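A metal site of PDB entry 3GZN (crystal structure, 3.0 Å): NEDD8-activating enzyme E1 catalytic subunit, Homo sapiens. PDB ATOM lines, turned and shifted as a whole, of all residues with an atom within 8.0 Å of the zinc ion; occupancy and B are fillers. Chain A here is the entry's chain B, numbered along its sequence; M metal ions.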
ATOM      1  N   ASN A 176      -2.566  -2.640 -32.453  1.00  0.00           N
ATOM      2  CA  ASN A 176      -2.792  -3.624 -31.399  1.00  0.00           C
ATOM      3  C   ASN A 176      -3.789  -3.116 -30.368  1.00  0.00           C
ATOM      4  O   ASN A 176      -4.758  -3.807 -30.035  1.00  0.00           O
ATOM      5  CB  ASN A 176      -1.478  -3.905 -30.702  1.00  0.00           C
ATOM      6  CG  ASN A 176      -1.547  -5.095 -29.802  1.00  0.00           C
ATOM      7  OD1 ASN A 176      -1.757  -6.226 -30.253  1.00  0.00           O
ATOM      8  ND2 ASN A 176      -1.357  -4.873 -28.507  1.00  0.00           N
ATOM      9  N   ILE A 180      -7.917  -4.128 -29.452  1.00  0.00           N
ATOM     10  CA  ILE A 180      -8.193  -4.564 -28.071  1.00  0.00           C
ATOM     11  C   ILE A 180      -9.276  -3.677 -27.456  1.00  0.00           C
ATOM     12  O   ILE A 180     -10.080  -4.142 -26.632  1.00  0.00           O
ATOM     13  CB  ILE A 180      -6.887  -4.526 -27.196  1.00  0.00           C
ATOM     14  CG1 ILE A 180      -6.005  -5.736 -27.509  1.00  0.00           C
ATOM     15  CG2 ILE A 180      -7.216  -4.508 -25.708  1.00  0.00           C
ATOM     16  CD1 ILE A 180      -4.527  -5.487 -27.220  1.00  0.00           C
ATOM     17  N   ILE A 213      -2.669 -12.778 -34.279  1.00  0.00           N
ATOM     18  CA  ILE A 213      -3.138 -12.302 -32.977  1.00  0.00           C
ATOM     19  C   ILE A 213      -4.676 -12.294 -32.887  1.00  0.00           C
ATOM     20  O   ILE A 213      -5.360 -11.843 -33.813  1.00  0.00           O
ATOM     21  CB  ILE A 213      -2.630 -10.881 -32.680  1.00  0.00           C
ATOM     22  CG1 ILE A 213      -1.108 -10.824 -32.730  1.00  0.00           C
ATOM     23  CG2 ILE A 213      -3.126 -10.426 -31.322  1.00  0.00           C
ATOM     24  CD1 ILE A 213      -0.555  -9.422 -32.812  1.00  0.00           C
ATOM     25  N   PRO A 215      -7.087 -10.653 -30.364  1.00  0.00           N
ATOM     26  CA  PRO A 215      -7.110  -9.775 -29.192  1.00  0.00           C
ATOM     27  C   PRO A 215      -7.967 -10.364 -28.088  1.00  0.00           C
ATOM     28  O   PRO A 215      -9.095 -10.788 -28.351  1.00  0.00           O
ATOM     29  CB  PRO A 215      -7.713  -8.477 -29.749  1.00  0.00           C
ATOM     30  CG  PRO A 215      -7.341  -8.496 -31.190  1.00  0.00           C
ATOM     31  CD  PRO A 215      -7.425  -9.942 -31.607  1.00  0.00           C
ATOM     32  N   GLY A 216      -7.412 -10.412 -26.876  1.00  0.00           N
ATOM     33  CA  GLY A 216      -8.104 -10.974 -25.716  1.00  0.00           C
ATOM     34  C   GLY A 216      -8.178 -12.498 -25.665  1.00  0.00           C
ATOM     35  O   GLY A 216      -8.934 -13.060 -24.883  1.00  0.00           O
ATOM     36  N   THR A 218      -5.218 -14.640 -27.549  1.00  0.00           N
ATOM     37  CA  THR A 218      -3.816 -15.050 -27.722  1.00  0.00           C
ATOM     38  C   THR A 218      -2.878 -13.863 -27.549  1.00  0.00           C
ATOM     39  O   THR A 218      -3.321 -12.714 -27.422  1.00  0.00           O
ATOM     40  CB  THR A 218      -3.583 -15.733 -29.087  1.00  0.00           C
ATOM     41  OG1 THR A 218      -4.076 -14.895 -30.146  1.00  0.00           O
ATOM     42  CG2 THR A 218      -4.252 -17.115 -29.133  1.00  0.00           C
ATOM     43  N   ALA A 219      -1.571 -14.156 -27.516  1.00  0.00           N
ATOM     44  CA  ALA A 219      -0.549 -13.133 -27.266  1.00  0.00           C
ATOM     45  C   ALA A 219      -0.660 -12.012 -28.262  1.00  0.00           C
ATOM     46  O   ALA A 219      -0.735 -12.261 -29.478  1.00  0.00           O
ATOM     47  CB  ALA A 219       0.859 -13.755 -27.307  1.00  0.00           C
ATOM     48  N   CYS A 220      -0.676 -10.784 -27.758  1.00  0.00           N
ATOM     49  CA  CYS A 220      -0.777  -9.607 -28.609  1.00  0.00           C
ATOM     50  C   CYS A 220       0.615  -8.999 -28.877  1.00  0.00           C
ATOM     51  O   CYS A 220       1.614  -9.510 -28.384  1.00  0.00           O
ATOM     52  CB  CYS A 220      -1.727  -8.574 -27.997  1.00  0.00           C
ATOM     53  SG  CYS A 220      -1.048  -7.569 -26.692  1.00  0.00           S
ATOM     54  N   ILE A 221       0.648  -7.929 -29.659  1.00  0.00           N
ATOM     55  CA  ILE A 221       1.900  -7.237 -29.993  1.00  0.00           C
ATOM     56  C   ILE A 221       2.709  -6.946 -28.730  1.00  0.00           C
ATOM     57  O   ILE A 221       3.917  -7.256 -28.677  1.00  0.00           O
ATOM     58  CB  ILE A 221       1.613  -5.922 -30.813  1.00  0.00           C
ATOM     59  CG1 ILE A 221       0.940  -6.226 -32.168  1.00  0.00           C
ATOM     60  CG2 ILE A 221       2.885  -5.049 -30.965  1.00  0.00           C
ATOM     61  CD1 ILE A 221       1.870  -6.649 -33.273  1.00  0.00           C
ATOM     62  N   GLU A 222       2.054  -6.389 -27.714  1.00  0.00           N
ATOM     63  CA  GLU A 222       2.702  -5.960 -26.469  1.00  0.00           C
ATOM     64  C   GLU A 222       3.136  -7.101 -25.554  1.00  0.00           C
ATOM     65  O   GLU A 222       4.134  -6.969 -24.841  1.00  0.00           O
ATOM     66  CB  GLU A 222       1.766  -5.049 -25.698  1.00  0.00           C
ATOM     67  CG  GLU A 222       1.477  -3.750 -26.403  1.00  0.00           C
ATOM     68  CD  GLU A 222       2.348  -2.596 -25.947  1.00  0.00           C
ATOM     69  OE1 GLU A 222       3.245  -2.811 -25.083  1.00  0.00           O
ATOM     70  OE2 GLU A 222       2.122  -1.470 -26.446  1.00  0.00           O
ATOM     71  N   CYS A 223       2.385  -8.207 -25.560  1.00  0.00           N
ATOM     72  CA  CYS A 223       2.785  -9.447 -24.901  1.00  0.00           C
ATOM     73  C   CYS A 223       4.188  -9.881 -25.322  1.00  0.00           C
ATOM     74  O   CYS A 223       4.989 -10.330 -24.492  1.00  0.00           O
ATOM     75  CB  CYS A 223       1.809 -10.574 -25.242  1.00  0.00           C
ATOM     76  SG  CYS A 223       0.175 -10.454 -24.537  1.00  0.00           S
ATOM     77  N   THR A 224       4.486  -9.765 -26.621  1.00  0.00           N
ATOM     78  CA  THR A 224       5.779 -10.156 -27.172  1.00  0.00           C
ATOM     79  C   THR A 224       6.647  -8.942 -27.545  1.00  0.00           C
ATOM     80  O   THR A 224       7.467  -9.032 -28.448  1.00  0.00           O
ATOM     81  CB  THR A 224       5.625 -11.096 -28.404  1.00  0.00           C
ATOM     82  OG1 THR A 224       4.748 -10.499 -29.365  1.00  0.00           O
ATOM     83  CG2 THR A 224       5.075 -12.452 -28.004  1.00  0.00           C
ATOM     84  N   LEU A 225       6.475  -7.828 -26.844  1.00  0.00           N
ATOM     85  CA  LEU A 225       7.169  -6.582 -27.210  1.00  0.00           C
ATOM     86  C   LEU A 225       8.685  -6.676 -27.114  1.00  0.00           C
ATOM     87  O   LEU A 225       9.417  -6.104 -27.922  1.00  0.00           O
ATOM     88  CB  LEU A 225       6.647  -5.419 -26.377  1.00  0.00           C
ATOM     89  CG  LEU A 225       7.183  -4.044 -26.758  1.00  0.00           C
ATOM     90  CD1 LEU A 225       6.902  -3.780 -28.224  1.00  0.00           C
ATOM     91  CD2 LEU A 225       6.588  -2.940 -25.884  1.00  0.00           C
ATOM     92  N   GLU A 359       3.071 -17.380 -25.722  1.00  0.00           N
ATOM     93  CA  GLU A 359       2.234 -17.340 -24.544  1.00  0.00           C
ATOM     94  C   GLU A 359       1.756 -15.912 -24.309  1.00  0.00           C
ATOM     95  O   GLU A 359       2.519 -14.966 -24.412  1.00  0.00           O
ATOM     96  CB  GLU A 359       3.021 -17.867 -23.334  1.00  0.00           C
ATOM     97  CG  GLU A 359       2.207 -18.043 -22.022  1.00  0.00           C
ATOM     98  CD  GLU A 359       3.086 -18.026 -20.750  1.00  0.00           C
ATOM     99  OE1 GLU A 359       4.191 -17.427 -20.766  1.00  0.00           O
ATOM    100  OE2 GLU A 359       2.653 -18.603 -19.726  1.00  0.00           O
ATOM    101  N   ARG A 360       0.468 -15.775 -24.000  1.00  0.00           N
ATOM    102  CA  ARG A 360      -0.106 -14.500 -23.600  1.00  0.00           C
ATOM    103  C   ARG A 360       0.424 -14.121 -22.225  1.00  0.00           C
ATOM    104  O   ARG A 360       0.519 -14.980 -21.347  1.00  0.00           O
ATOM    105  CB  ARG A 360      -1.614 -14.648 -23.553  1.00  0.00           C
ATOM    106  CG  ARG A 360      -2.395 -13.359 -23.354  1.00  0.00           C
ATOM    107  CD  ARG A 360      -3.890 -13.697 -23.635  1.00  0.00           C
ATOM    108  NE  ARG A 360      -4.734 -12.523 -23.514  1.00  0.00           N
ATOM    109  CZ  ARG A 360      -5.621 -12.334 -22.515  1.00  0.00           C
ATOM    110  NH1 ARG A 360      -5.790 -13.241 -21.564  1.00  0.00           N
ATOM    111  NH2 ARG A 360      -6.346 -11.213 -22.498  1.00  0.00           N
ATOM    112  N   LYS A 361       0.789 -12.864 -22.031  1.00  0.00           N
ATOM    113  CA  LYS A 361       1.198 -12.401 -20.699  1.00  0.00           C
ATOM    114  C   LYS A 361      -0.006 -12.030 -19.822  1.00  0.00           C
ATOM    115  O   LYS A 361      -0.801 -11.146 -20.208  1.00  0.00           O
ATOM    116  CB  LYS A 361       2.202 -11.259 -20.764  1.00  0.00           C
ATOM    117  CG  LYS A 361       3.618 -11.735 -21.058  1.00  0.00           C
ATOM    118  CD  LYS A 361       4.637 -10.625 -20.854  1.00  0.00           C
ATOM    119  CE  LYS A 361       6.048 -11.177 -20.938  1.00  0.00           C
ATOM    120  NZ  LYS A 361       7.052 -10.082 -21.106  1.00  0.00           N
ATOM    121  N   GLU A 362      -0.142 -12.700 -18.681  1.00  0.00           N
ATOM    122  CA  GLU A 362      -1.301 -12.502 -17.773  1.00  0.00           C
ATOM    123  C   GLU A 362      -1.393 -11.062 -17.251  1.00  0.00           C
ATOM    124  O   GLU A 362      -2.492 -10.535 -17.047  1.00  0.00           O
ATOM    125  CB  GLU A 362      -1.293 -13.516 -16.614  1.00  0.00           C
ATOM    126  N   ASN A 363      -0.226 -10.432 -17.100  1.00  0.00           N
ATOM    127  CA  ASN A 363      -0.078  -9.056 -16.655  1.00  0.00           C
ATOM    128  C   ASN A 363      -0.068  -7.973 -17.734  1.00  0.00           C
ATOM    129  O   ASN A 363       0.060  -6.790 -17.412  1.00  0.00           O
ATOM    130  CB  ASN A 363       1.250  -8.944 -15.893  1.00  0.00           C
ATOM    131  CG  ASN A 363       1.152  -9.487 -14.468  1.00  0.00           C
ATOM    132  OD1 ASN A 363       2.168  -9.929 -13.897  1.00  0.00           O
ATOM    133  ND2 ASN A 363      -0.048  -9.445 -13.898  1.00  0.00           N
ATOM    134  N   CYS A 364      -0.185  -8.360 -19.010  1.00  0.00           N
ATOM    135  CA  CYS A 364       0.056  -7.434 -20.135  1.00  0.00           C
ATOM    136  C   CYS A 364      -0.653  -6.079 -19.993  1.00  0.00           C
ATOM    137  O   CYS A 364      -1.857  -6.038 -19.716  1.00  0.00           O
ATOM    138  CB  CYS A 364      -0.314  -8.096 -21.462  1.00  0.00           C
ATOM    139  SG  CYS A 364      -0.002  -7.108 -22.966  1.00  0.00           S
ATOM    140  N   PRO A 365       0.088  -4.973 -20.181  1.00  0.00           N
ATOM    141  CA  PRO A 365      -0.499  -3.638 -19.996  1.00  0.00           C
ATOM    142  C   PRO A 365      -1.487  -3.273 -21.100  1.00  0.00           C
ATOM    143  O   PRO A 365      -2.170  -2.254 -20.996  1.00  0.00           O
ATOM    144  CB  PRO A 365       0.715  -2.694 -20.048  1.00  0.00           C
ATOM    145  CG  PRO A 365       1.925  -3.570 -20.044  1.00  0.00           C
ATOM    146  CD  PRO A 365       1.502  -4.904 -20.579  1.00  0.00           C
ATOM    147  N   ALA A 366      -1.554  -4.107 -22.135  1.00  0.00           N
ATOM    148  CA  ALA A 366      -2.414  -3.834 -23.266  1.00  0.00           C
ATOM    149  C   ALA A 366      -3.642  -4.725 -23.265  1.00  0.00           C
ATOM    150  O   ALA A 366      -4.771  -4.233 -23.238  1.00  0.00           O
ATOM    151  CB  ALA A 366      -1.650  -3.998 -24.566  1.00  0.00           C
ATOM    152  N   CYS A 367      -3.423  -6.033 -23.281  1.00  0.00           N
ATOM    153  CA  CYS A 367      -4.514  -6.952 -23.543  1.00  0.00           C
ATOM    154  C   CYS A 367      -5.187  -7.561 -22.310  1.00  0.00           C
ATOM    155  O   CYS A 367      -6.325  -8.008 -22.422  1.00  0.00           O
ATOM    156  CB  CYS A 367      -4.091  -8.052 -24.535  1.00  0.00           C
ATOM    157  SG  CYS A 367      -2.865  -9.195 -23.928  1.00  0.00           S
ATOM    158  N   SER A 368      -4.516  -7.563 -21.171  1.00  0.00           N
ATOM    159  CA  SER A 368      -5.132  -8.093 -19.950  1.00  0.00           C
ATOM    160  C   SER A 368      -6.142  -7.096 -19.382  1.00  0.00           C
ATOM    161  O   SER A 368      -6.035  -5.896 -19.629  1.00  0.00           O
ATOM    162  CB  SER A 368      -4.082  -8.456 -18.897  1.00  0.00           C
ATOM    163  OG  SER A 368      -3.780  -7.339 -18.071  1.00  0.00           O
HETATM  164 ZN    ZN M   1      -0.966  -8.642 -24.411  1.00  0.00          ZN
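Four residues have an atom within 4 Å of the zinc ion: Cys 220, Cys 223, Cys 364 and Cys 367. Along chain A the residues within 4 Å of the zinc ion span positions 220 to 367. The nearest printed residue that does not touch the zinc ion is Glu 222 (4.5 Å).
The zinc ion is bound by the side-chain sulfur of Cys 367, the side-chain sulfur of Cys 223, the side-chain sulfur of Cys 364 and the side-chain sulfur of Cys 220.
The guanidinium group (NH2) of Arg 360 is in hydrogen-bond range of the backbone carbonyl oxygen (O) of Cys 367, at 3.2 Å. SG of Cys 223 sits close to N of Lys 361 (3.5 Å). The side-chain sulfur (SG) of Cys 364 lies close to the backbone NH (N) of Ala 366 (3.5 Å). OG of Ser 368 sits at hydrogen-bond distance from O of Cys 364 (2.8 Å). The side-chain sulfur of Cys 220 sits close to the backbone NH of Glu 222 (3.5 Å). The side-chain amide nitrogen (ND2) of Asn 176 sits close to the side-chain sulfur (SG) of Cys 220. O of Cys 220 is in hydrogen-bond range of OG1 of Thr 224, 3.4 Å away.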
